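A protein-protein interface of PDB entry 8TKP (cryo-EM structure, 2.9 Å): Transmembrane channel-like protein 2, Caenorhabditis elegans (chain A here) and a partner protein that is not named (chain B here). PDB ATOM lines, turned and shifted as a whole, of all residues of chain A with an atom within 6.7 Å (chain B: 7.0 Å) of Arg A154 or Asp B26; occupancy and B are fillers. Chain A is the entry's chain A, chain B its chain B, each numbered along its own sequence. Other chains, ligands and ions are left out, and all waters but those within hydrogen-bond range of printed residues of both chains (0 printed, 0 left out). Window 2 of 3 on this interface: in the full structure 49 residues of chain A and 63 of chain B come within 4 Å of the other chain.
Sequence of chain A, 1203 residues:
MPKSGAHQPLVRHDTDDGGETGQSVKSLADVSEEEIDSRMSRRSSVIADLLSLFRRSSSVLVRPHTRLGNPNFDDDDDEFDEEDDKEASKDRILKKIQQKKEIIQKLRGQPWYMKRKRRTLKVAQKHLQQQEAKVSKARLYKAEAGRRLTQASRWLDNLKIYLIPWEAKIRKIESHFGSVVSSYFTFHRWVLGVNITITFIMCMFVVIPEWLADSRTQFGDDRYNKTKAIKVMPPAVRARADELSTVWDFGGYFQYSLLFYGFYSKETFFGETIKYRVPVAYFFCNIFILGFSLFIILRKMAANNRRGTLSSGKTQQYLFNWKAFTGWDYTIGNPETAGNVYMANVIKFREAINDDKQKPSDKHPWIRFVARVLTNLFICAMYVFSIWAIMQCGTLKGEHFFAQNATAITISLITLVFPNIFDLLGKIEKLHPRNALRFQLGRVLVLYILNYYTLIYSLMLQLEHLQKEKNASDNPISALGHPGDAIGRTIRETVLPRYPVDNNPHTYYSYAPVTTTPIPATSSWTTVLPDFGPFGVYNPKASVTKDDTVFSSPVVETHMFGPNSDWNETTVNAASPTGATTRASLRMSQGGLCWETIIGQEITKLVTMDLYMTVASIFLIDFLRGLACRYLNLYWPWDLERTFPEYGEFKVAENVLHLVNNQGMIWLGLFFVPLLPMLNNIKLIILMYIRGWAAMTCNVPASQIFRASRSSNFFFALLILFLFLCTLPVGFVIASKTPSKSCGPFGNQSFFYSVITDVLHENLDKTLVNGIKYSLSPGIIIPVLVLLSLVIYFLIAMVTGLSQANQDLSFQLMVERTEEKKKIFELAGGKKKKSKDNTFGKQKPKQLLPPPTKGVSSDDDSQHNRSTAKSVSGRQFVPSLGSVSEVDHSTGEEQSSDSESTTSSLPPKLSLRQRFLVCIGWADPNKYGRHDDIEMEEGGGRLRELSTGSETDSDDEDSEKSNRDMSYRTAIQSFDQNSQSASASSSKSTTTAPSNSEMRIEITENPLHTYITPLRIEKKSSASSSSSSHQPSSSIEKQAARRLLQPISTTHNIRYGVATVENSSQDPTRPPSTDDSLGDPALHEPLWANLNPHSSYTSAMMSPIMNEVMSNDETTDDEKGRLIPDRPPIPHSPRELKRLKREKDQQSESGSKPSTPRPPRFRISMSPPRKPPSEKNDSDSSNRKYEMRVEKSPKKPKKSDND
NH2 of Arg A108 lies within hydrogen-bond range of O of Gln B29 (3.4 Å). The side-chain carboxylate (OD1) of Asp B26 is in salt-bridge range of the guanidinium group (NH1) of Arg A154. The guanidinium group of Arg A154 is in salt-bridge range of the side-chain carboxylate of Asp B30, 2.5 Å away. ND2 of Asn A158 sits at hydrogen-bond distance from OE1 of Gln B29 (2.9 Å).
OE1 of Gln A125 lies close to O of Leu A121, 3.3 Å away. The backbone carbonyl oxygen (O) of Arg A154 lies close to the side-chain amide nitrogen (ND2) of Asn A158, 3.3 Å away. O of Glu B27 is in hydrogen-bond range of SG of Cys B31, 3.3 Å away. The side-chain hydroxyl (OG1) of Thr B32 sits at hydrogen-bond distance from the backbone carbonyl oxygen (O) of Tyr B28 (3.0 Å).
Asp B30 touches Arg A108 (O to CB, 3.9 Å). NE of Arg A108 touches O of Thr B32, 3.5 Å away. Leu A121 touches Asp B30 (CD2 to CB, 3.7 Å). Leu A121 touches Cys B31 (CD2 to SG, 3.8 Å). Gln B29 touches Arg A154. CB of Thr B35 touches OD1 of Asn A158 (3.3 Å).
Arg A154 touches three residues of chain B. Asp B26 touches one residue of chain A. Of the printed residues of chain A, Gln B29 touches Arg A108 (3.4 Å), Arg A154 (3.7 Å) and Asn A158 (2.9 Å). Printed residues of chain A within 4 Å of Asp B30: Arg A108 (3.9 Å), Leu A121 (3.7 Å) and Arg A154 (2.5 Å). Of the printed residues of chain A, Cys B31 touches Leu A121 (3.8 Å). Ile B39 touches none of the printed residues of chain A. The nearest residue of chain B that does not touch Arg A154 is Glu B27 (5.7 Å). The nearest printed residue of chain A that does not touch Cys B31 is Arg A108 (4.2 Å).
Among the printed residues, 10 pairs touch across the chains.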
ATOM      1  N   ARG A 108      33.004  -8.218  25.936  1.00  0.00           N
ATOM      2  CA  ARG A 108      32.069  -7.856  24.875  1.00  0.00           C
ATOM      3  C   ARG A 108      32.494  -6.602  24.120  1.00  0.00           C
ATOM      4  O   ARG A 108      32.173  -6.467  22.935  1.00  0.00           O
ATOM      5  CB  ARG A 108      30.667  -7.669  25.460  1.00  0.00           C
ATOM      6  CG  ARG A 108      29.588  -7.384  24.429  1.00  0.00           C
ATOM      7  CD  ARG A 108      28.206  -7.313  25.059  1.00  0.00           C
ATOM      8  NE  ARG A 108      27.727  -8.620  25.491  1.00  0.00           N
ATOM      9  CZ  ARG A 108      27.762  -9.056  26.742  1.00  0.00           C
ATOM     10  NH1 ARG A 108      28.247  -8.308  27.720  1.00  0.00           N
ATOM     11  NH2 ARG A 108      27.296 -10.270  27.020  1.00  0.00           N
ATOM     12  N   LEU A 121      37.411 -15.988  26.339  1.00  0.00           N
ATOM     13  CA  LEU A 121      36.192 -16.475  26.971  1.00  0.00           C
ATOM     14  C   LEU A 121      36.356 -17.910  27.450  1.00  0.00           C
ATOM     15  O   LEU A 121      35.967 -18.244  28.574  1.00  0.00           O
ATOM     16  CB  LEU A 121      35.021 -16.368  25.993  1.00  0.00           C
ATOM     17  CG  LEU A 121      33.636 -16.726  26.533  1.00  0.00           C
ATOM     18  CD1 LEU A 121      33.145 -15.657  27.494  1.00  0.00           C
ATOM     19  CD2 LEU A 121      32.651 -16.923  25.392  1.00  0.00           C
ATOM     20  N   GLN A 125      36.267 -18.990  31.366  1.00  0.00           N
ATOM     21  CA  GLN A 125      35.261 -19.946  31.817  1.00  0.00           C
ATOM     22  C   GLN A 125      35.907 -21.177  32.442  1.00  0.00           C
ATOM     23  O   GLN A 125      35.426 -21.691  33.461  1.00  0.00           O
ATOM     24  CB  GLN A 125      34.354 -20.339  30.652  1.00  0.00           C
ATOM     25  CG  GLN A 125      33.414 -19.231  30.207  1.00  0.00           C
ATOM     26  CD  GLN A 125      32.812 -19.490  28.841  1.00  0.00           C
ATOM     27  OE1 GLN A 125      33.410 -20.168  28.005  1.00  0.00           O
ATOM     28  NE2 GLN A 125      31.623 -18.950  28.606  1.00  0.00           N
ATOM     29  N   LEU A 149      20.005 -16.464  37.111  1.00  0.00           N
ATOM     30  CA  LEU A 149      19.384 -15.165  36.881  1.00  0.00           C
ATOM     31  C   LEU A 149      19.978 -14.475  35.660  1.00  0.00           C
ATOM     32  O   LEU A 149      19.255 -13.849  34.880  1.00  0.00           O
ATOM     33  CB  LEU A 149      19.537 -14.286  38.123  1.00  0.00           C
ATOM     34  CG  LEU A 149      18.938 -12.881  38.046  1.00  0.00           C
ATOM     35  CD1 LEU A 149      17.440 -12.950  37.799  1.00  0.00           C
ATOM     36  CD2 LEU A 149      19.241 -12.101  39.316  1.00  0.00           C
ATOM     37  N   THR A 150      21.298 -14.569  35.485  1.00  0.00           N
ATOM     38  CA  THR A 150      21.923 -14.003  34.293  1.00  0.00           C
ATOM     39  C   THR A 150      21.419 -14.695  33.031  1.00  0.00           C
ATOM     40  O   THR A 150      21.127 -14.037  32.021  1.00  0.00           O
ATOM     41  CB  THR A 150      23.444 -14.114  34.393  1.00  0.00           C
ATOM     42  OG1 THR A 150      23.902 -13.402  35.549  1.00  0.00           O
ATOM     43  CG2 THR A 150      24.107 -13.532  33.154  1.00  0.00           C
ATOM     44  N   GLN A 151      21.304 -16.025  33.072  1.00  0.00           N
ATOM     45  CA  GLN A 151      20.773 -16.757  31.927  1.00  0.00           C
ATOM     46  C   GLN A 151      19.337 -16.339  31.627  1.00  0.00           C
ATOM     47  O   GLN A 151      18.962 -16.163  30.462  1.00  0.00           O
ATOM     48  CB  GLN A 151      20.858 -18.262  32.185  1.00  0.00           C
ATOM     49  CG  GLN A 151      20.410 -19.136  31.018  1.00  0.00           C
ATOM     50  CD  GLN A 151      18.922 -19.434  31.040  1.00  0.00           C
ATOM     51  OE1 GLN A 151      18.247 -19.215  32.046  1.00  0.00           O
ATOM     52  NE2 GLN A 151      18.401 -19.933  29.925  1.00  0.00           N
ATOM     53  N   ALA A 152      18.521 -16.176  32.671  1.00  0.00           N
ATOM     54  CA  ALA A 152      17.140 -15.748  32.478  1.00  0.00           C
ATOM     55  C   ALA A 152      17.073 -14.341  31.903  1.00  0.00           C
ATOM     56  O   ALA A 152      16.211 -14.046  31.068  1.00  0.00           O
ATOM     57  CB  ALA A 152      16.377 -15.827  33.799  1.00  0.00           C
ATOM     58  N   SER A 153      17.962 -13.453  32.348  1.00  0.00           N
ATOM     59  CA  SER A 153      17.998 -12.099  31.807  1.00  0.00           C
ATOM     60  C   SER A 153      18.347 -12.115  30.325  1.00  0.00           C
ATOM     61  O   SER A 153      17.725 -11.413  29.519  1.00  0.00           O
ATOM     62  CB  SER A 153      18.999 -11.247  32.588  1.00  0.00           C
ATOM     63  OG  SER A 153      20.313 -11.759  32.456  1.00  0.00           O
ATOM     64  N   ARG A 154      19.342 -12.920  29.946  1.00  0.00           N
ATOM     65  CA  ARG A 154      19.689 -13.032  28.532  1.00  0.00           C
ATOM     66  C   ARG A 154      18.529 -13.602  27.725  1.00  0.00           C
ATOM     67  O   ARG A 154      18.237 -13.130  26.618  1.00  0.00           O
ATOM     68  CB  ARG A 154      20.942 -13.891  28.363  1.00  0.00           C
ATOM     69  CG  ARG A 154      21.258 -14.239  26.919  1.00  0.00           C
ATOM     70  CD  ARG A 154      22.654 -14.819  26.783  1.00  0.00           C
ATOM     71  NE  ARG A 154      23.680 -13.832  27.095  1.00  0.00           N
ATOM     72  CZ  ARG A 154      24.984 -14.060  27.027  1.00  0.00           C
ATOM     73  NH1 ARG A 154      25.462 -15.237  26.660  1.00  0.00           N
ATOM     74  NH2 ARG A 154      25.830 -13.081  27.332  1.00  0.00           N
ATOM     75  N   TRP A 155      17.853 -14.617  28.268  1.00  0.00           N
ATOM     76  CA  TRP A 155      16.719 -15.213  27.570  1.00  0.00           C
ATOM     77  C   TRP A 155      15.587 -14.210  27.388  1.00  0.00           C
ATOM     78  O   TRP A 155      14.978 -14.137  26.313  1.00  0.00           O
ATOM     79  CB  TRP A 155      16.229 -16.444  28.332  1.00  0.00           C
ATOM     80  CG  TRP A 155      14.966 -17.028  27.788  1.00  0.00           C
ATOM     81  CD1 TRP A 155      14.852 -17.959  26.798  1.00  0.00           C
ATOM     82  CD2 TRP A 155      13.631 -16.724  28.206  1.00  0.00           C
ATOM     83  NE1 TRP A 155      13.530 -18.252  26.573  1.00  0.00           N
ATOM     84  CE2 TRP A 155      12.759 -17.506  27.425  1.00  0.00           C
ATOM     85  CE3 TRP A 155      13.089 -15.863  29.166  1.00  0.00           C
ATOM     86  CZ2 TRP A 155      11.375 -17.454  27.574  1.00  0.00           C
ATOM     87  CZ3 TRP A 155      11.715 -15.812  29.312  1.00  0.00           C
ATOM     88  CH2 TRP A 155      10.874 -16.604  28.520  1.00  0.00           C
ATOM     89  N   LEU A 156      15.290 -13.423  28.424  1.00  0.00           N
ATOM     90  CA  LEU A 156      14.209 -12.450  28.311  1.00  0.00           C
ATOM     91  C   LEU A 156      14.583 -11.323  27.358  1.00  0.00           C
ATOM     92  O   LEU A 156      13.720 -10.800  26.647  1.00  0.00           O
ATOM     93  CB  LEU A 156      13.824 -11.910  29.692  1.00  0.00           C
ATOM     94  CG  LEU A 156      14.736 -10.982  30.500  1.00  0.00           C
ATOM     95  CD1 LEU A 156      14.534  -9.518  30.124  1.00  0.00           C
ATOM     96  CD2 LEU A 156      14.491 -11.184  31.987  1.00  0.00           C
ATOM     97  N   ASP A 157      15.861 -10.938  27.318  1.00  0.00           N
ATOM     98  CA  ASP A 157      16.293  -9.951  26.332  1.00  0.00           C
ATOM     99  C   ASP A 157      16.142 -10.488  24.913  1.00  0.00           C
ATOM    100  O   ASP A 157      15.693  -9.767  24.010  1.00  0.00           O
ATOM    101  CB  ASP A 157      17.740  -9.537  26.598  1.00  0.00           C
ATOM    102  CG  ASP A 157      17.900  -8.787  27.906  1.00  0.00           C
ATOM    103  OD1 ASP A 157      16.946  -8.093  28.314  1.00  0.00           O
ATOM    104  OD2 ASP A 157      18.980  -8.892  28.524  1.00  0.00           O
ATOM    105  N   ASN A 158      16.515 -11.751  24.696  1.00  0.00           N
ATOM    106  CA  ASN A 158      16.352 -12.352  23.377  1.00  0.00           C
ATOM    107  C   ASN A 158      14.880 -12.433  22.987  1.00  0.00           C
ATOM    108  O   ASN A 158      14.528 -12.244  21.818  1.00  0.00           O
ATOM    109  CB  ASN A 158      16.994 -13.740  23.344  1.00  0.00           C
ATOM    110  CG  ASN A 158      18.502 -13.686  23.470  1.00  0.00           C
ATOM    111  OD1 ASN A 158      19.122 -12.656  23.207  1.00  0.00           O
ATOM    112  ND2 ASN A 158      19.102 -14.802  23.867  1.00  0.00           N
ATOM    113  N   LEU A 159      14.009 -12.733  23.952  1.00  0.00           N
ATOM    114  CA  LEU A 159      12.577 -12.731  23.675  1.00  0.00           C
ATOM    115  C   LEU A 159      12.077 -11.325  23.356  1.00  0.00           C
ATOM    116  O   LEU A 159      11.243 -11.141  22.462  1.00  0.00           O
ATOM    117  CB  LEU A 159      11.813 -13.320  24.862  1.00  0.00           C
ATOM    118  CG  LEU A 159      10.291 -13.419  24.749  1.00  0.00           C
ATOM    119  CD1 LEU A 159       9.805 -14.741  25.317  1.00  0.00           C
ATOM    120  CD2 LEU A 159       9.613 -12.256  25.463  1.00  0.00           C
ATOM    121  N   THR B  21      24.611 -23.813  16.392  1.00  0.00           N
ATOM    122  CA  THR B  21      24.379 -24.563  17.617  1.00  0.00           C
ATOM    123  C   THR B  21      24.124 -23.599  18.767  1.00  0.00           C
ATOM    124  O   THR B  21      24.474 -22.418  18.700  1.00  0.00           O
ATOM    125  CB  THR B  21      25.573 -25.459  17.951  1.00  0.00           C
ATOM    126  OG1 THR B  21      26.686 -24.646  18.344  1.00  0.00           O
ATOM    127  CG2 THR B  21      25.966 -26.292  16.743  1.00  0.00           C
ATOM    128  N   ARG B  22      23.501 -24.115  19.828  1.00  0.00           N
ATOM    129  CA  ARG B  22      23.254 -23.294  21.007  1.00  0.00           C
ATOM    130  C   ARG B  22      24.560 -22.800  21.615  1.00  0.00           C
ATOM    131  O   ARG B  22      24.645 -21.661  22.087  1.00  0.00           O
ATOM    132  CB  ARG B  22      22.443 -24.077  22.040  1.00  0.00           C
ATOM    133  CG  ARG B  22      20.957 -23.747  22.049  1.00  0.00           C
ATOM    134  CD  ARG B  22      20.302 -24.060  20.714  1.00  0.00           C
ATOM    135  NE  ARG B  22      18.878 -23.746  20.717  1.00  0.00           N
ATOM    136  CZ  ARG B  22      18.064 -23.946  19.690  1.00  0.00           C
ATOM    137  NH1 ARG B  22      18.501 -24.465  18.554  1.00  0.00           N
ATOM    138  NH2 ARG B  22      16.780 -23.620  19.806  1.00  0.00           N
ATOM    139  N   GLU B  23      25.590 -23.648  21.613  1.00  0.00           N
ATOM    140  CA  GLU B  23      26.887 -23.234  22.134  1.00  0.00           C
ATOM    141  C   GLU B  23      27.476 -22.093  21.313  1.00  0.00           C
ATOM    142  O   GLU B  23      28.007 -21.129  21.874  1.00  0.00           O
ATOM    143  CB  GLU B  23      27.849 -24.423  22.163  1.00  0.00           C
ATOM    144  CG  GLU B  23      27.651 -25.363  23.342  1.00  0.00           C
ATOM    145  CD  GLU B  23      26.336 -26.114  23.285  1.00  0.00           C
ATOM    146  OE1 GLU B  23      25.771 -26.250  22.179  1.00  0.00           O
ATOM    147  OE2 GLU B  23      25.864 -26.568  24.349  1.00  0.00           O
ATOM    148  N   GLN B  24      27.389 -22.182  19.985  1.00  0.00           N
ATOM    149  CA  GLN B  24      27.932 -21.125  19.138  1.00  0.00           C
ATOM    150  C   GLN B  24      27.183 -19.814  19.342  1.00  0.00           C
ATOM    151  O   GLN B  24      27.794 -18.743  19.428  1.00  0.00           O
ATOM    152  CB  GLN B  24      27.888 -21.547  17.671  1.00  0.00           C
ATOM    153  CG  GLN B  24      28.971 -22.530  17.276  1.00  0.00           C
ATOM    154  CD  GLN B  24      29.126 -22.646  15.775  1.00  0.00           C
ATOM    155  OE1 GLN B  24      28.241 -23.149  15.084  1.00  0.00           O
ATOM    156  NE2 GLN B  24      30.254 -22.172  15.260  1.00  0.00           N
ATOM    157  N   LEU B  25      25.852 -19.878  19.413  1.00  0.00           N
ATOM    158  CA  LEU B  25      25.072 -18.663  19.621  1.00  0.00           C
ATOM    159  C   LEU B  25      25.356 -18.050  20.985  1.00  0.00           C
ATOM    160  O   LEU B  25      25.467 -16.826  21.108  1.00  0.00           O
ATOM    161  CB  LEU B  25      23.583 -18.963  19.459  1.00  0.00           C
ATOM    162  CG  LEU B  25      23.156 -19.353  18.044  1.00  0.00           C
ATOM    163  CD1 LEU B  25      21.669 -19.657  17.987  1.00  0.00           C
ATOM    164  CD2 LEU B  25      23.517 -18.254  17.058  1.00  0.00           C
ATOM    165  N   ASP B  26      25.478 -18.882  22.021  1.00  0.00           N
ATOM    166  CA  ASP B  26      25.818 -18.369  23.345  1.00  0.00           C
ATOM    167  C   ASP B  26      27.202 -17.734  23.348  1.00  0.00           C
ATOM    168  O   ASP B  26      27.408 -16.673  23.953  1.00  0.00           O
ATOM    169  CB  ASP B  26      25.737 -19.492  24.376  1.00  0.00           C
ATOM    170  CG  ASP B  26      25.828 -18.984  25.802  1.00  0.00           C
ATOM    171  OD1 ASP B  26      25.739 -17.756  26.006  1.00  0.00           O
ATOM    172  OD2 ASP B  26      25.990 -19.815  26.721  1.00  0.00           O
ATOM    173  N   GLU B  27      28.166 -18.366  22.674  1.00  0.00           N
ATOM    174  CA  GLU B  27      29.509 -17.805  22.590  1.00  0.00           C
ATOM    175  C   GLU B  27      29.501 -16.462  21.871  1.00  0.00           C
ATOM    176  O   GLU B  27      30.169 -15.515  22.302  1.00  0.00           O
ATOM    177  CB  GLU B  27      30.436 -18.792  21.884  1.00  0.00           C
ATOM    178  CG  GLU B  27      31.713 -18.183  21.342  1.00  0.00           C
ATOM    179  CD  GLU B  27      32.563 -19.194  20.601  1.00  0.00           C
ATOM    180  OE1 GLU B  27      33.014 -20.171  21.234  1.00  0.00           O
ATOM    181  OE2 GLU B  27      32.766 -19.020  19.382  1.00  0.00           O
ATOM    182  N   TYR B  28      28.748 -16.362  20.776  1.00  0.00           N
ATOM    183  CA  TYR B  28      28.653 -15.090  20.066  1.00  0.00           C
ATOM    184  C   TYR B  28      27.995 -14.023  20.928  1.00  0.00           C
ATOM    185  O   TYR B  28      28.465 -12.881  20.976  1.00  0.00           O
ATOM    186  CB  TYR B  28      27.891 -15.269  18.754  1.00  0.00           C
ATOM    187  CG  TYR B  28      28.748 -15.757  17.609  1.00  0.00           C
ATOM    188  CD1 TYR B  28      29.806 -14.994  17.138  1.00  0.00           C
ATOM    189  CD2 TYR B  28      28.491 -16.971  16.991  1.00  0.00           C
ATOM    190  CE1 TYR B  28      30.589 -15.432  16.089  1.00  0.00           C
ATOM    191  CE2 TYR B  28      29.268 -17.418  15.942  1.00  0.00           C
ATOM    192  CZ  TYR B  28      30.315 -16.642  15.495  1.00  0.00           C
ATOM    193  OH  TYR B  28      31.093 -17.083  14.450  1.00  0.00           O
ATOM    194  N   GLN B  29      26.917 -14.376  21.634  1.00  0.00           N
ATOM    195  CA  GLN B  29      26.262 -13.406  22.507  1.00  0.00           C
ATOM    196  C   GLN B  29      27.199 -12.942  23.614  1.00  0.00           C
ATOM    197  O   GLN B  29      27.157 -11.776  24.024  1.00  0.00           O
ATOM    198  CB  GLN B  29      24.986 -14.004  23.098  1.00  0.00           C
ATOM    199  CG  GLN B  29      23.865 -14.190  22.095  1.00  0.00           C
ATOM    200  CD  GLN B  29      22.598 -14.722  22.733  1.00  0.00           C
ATOM    201  OE1 GLN B  29      21.800 -13.964  23.282  1.00  0.00           O
ATOM    202  NE2 GLN B  29      22.409 -16.035  22.667  1.00  0.00           N
ATOM    203  N   ASP B  30      28.037 -13.843  24.123  1.00  0.00           N
ATOM    204  CA  ASP B  30      29.045 -13.440  25.097  1.00  0.00           C
ATOM    205  C   ASP B  30      30.070 -12.501  24.472  1.00  0.00           C
ATOM    206  O   ASP B  30      30.496 -11.527  25.103  1.00  0.00           O
ATOM    207  CB  ASP B  30      29.734 -14.671  25.684  1.00  0.00           C
ATOM    208  CG  ASP B  30      28.792 -15.532  26.499  1.00  0.00           C
ATOM    209  OD1 ASP B  30      27.895 -14.971  27.160  1.00  0.00           O
ATOM    210  OD2 ASP B  30      28.949 -16.772  26.479  1.00  0.00           O
ATOM    211  N   CYS B  31      30.475 -12.775  23.234  1.00  0.00           N
ATOM    212  CA  CYS B  31      31.526 -12.014  22.573  1.00  0.00           C
ATOM    213  C   CYS B  31      31.001 -10.895  21.680  1.00  0.00           C
ATOM    214  O   CYS B  31      31.808 -10.195  21.058  1.00  0.00           O
ATOM    215  CB  CYS B  31      32.406 -12.953  21.742  1.00  0.00           C
ATOM    216  SG  CYS B  31      33.166 -14.291  22.688  1.00  0.00           S
ATOM    217  N   THR B  32      29.686 -10.703  21.596  1.00  0.00           N
ATOM    218  CA  THR B  32      29.122  -9.712  20.691  1.00  0.00           C
ATOM    219  C   THR B  32      27.869  -9.121  21.320  1.00  0.00           C
ATOM    220  O   THR B  32      27.247  -9.725  22.197  1.00  0.00           O
ATOM    221  CB  THR B  32      28.799 -10.328  19.321  1.00  0.00           C
ATOM    222  OG1 THR B  32      29.852 -11.219  18.935  1.00  0.00           O
ATOM    223  CG2 THR B  32      28.658  -9.260  18.262  1.00  0.00           C
ATOM    224  N   THR B  35      21.907 -10.272  19.656  1.00  0.00           N
ATOM    225  CA  THR B  35      21.095 -11.365  20.157  1.00  0.00           C
ATOM    226  C   THR B  35      21.065 -12.480  19.115  1.00  0.00           C
ATOM    227  O   THR B  35      21.693 -12.392  18.059  1.00  0.00           O
ATOM    228  CB  THR B  35      19.686 -10.876  20.488  1.00  0.00           C
ATOM    229  OG1 THR B  35      19.040 -10.435  19.288  1.00  0.00           O
ATOM    230  CG2 THR B  35      19.747  -9.720  21.472  1.00  0.00           C
ATOM    231  N   ARG B  36      20.324 -13.551  19.411  1.00  0.00           N
ATOM    232  CA  ARG B  36      20.231 -14.659  18.466  1.00  0.00           C
ATOM    233  C   ARG B  36      19.581 -14.215  17.161  1.00  0.00           C
ATOM    234  O   ARG B  36      20.026 -14.594  16.071  1.00  0.00           O
ATOM    235  CB  ARG B  36      19.453 -15.818  19.090  1.00  0.00           C
ATOM    236  CG  ARG B  36      20.200 -16.536  20.199  1.00  0.00           C
ATOM    237  CD  ARG B  36      19.395 -17.705  20.741  1.00  0.00           C
ATOM    238  NE  ARG B  36      18.995 -18.625  19.683  1.00  0.00           N
ATOM    239  CZ  ARG B  36      18.421 -19.802  19.892  1.00  0.00           C
ATOM    240  NH1 ARG B  36      18.167 -20.240  21.114  1.00  0.00           N
ATOM    241  NH2 ARG B  36      18.091 -20.558  18.848  1.00  0.00           N
ATOM    242  N   ILE B  39      22.059 -12.203  15.064  1.00  0.00           N
ATOM    243  CA  ILE B  39      23.073 -13.073  14.473  1.00  0.00           C
ATOM    244  C   ILE B  39      22.495 -13.844  13.295  1.00  0.00           C
ATOM    245  O   ILE B  39      23.138 -13.984  12.248  1.00  0.00           O
ATOM    246  CB  ILE B  39      23.653 -14.017  15.540  1.00  0.00           C
ATOM    247  CG1 ILE B  39      24.360 -13.215  16.631  1.00  0.00           C
ATOM    248  CG2 ILE B  39      24.614 -15.010  14.911  1.00  0.00           C
ATOM    249  CD1 ILE B  39      24.646 -14.011  17.878  1.00  0.00           C
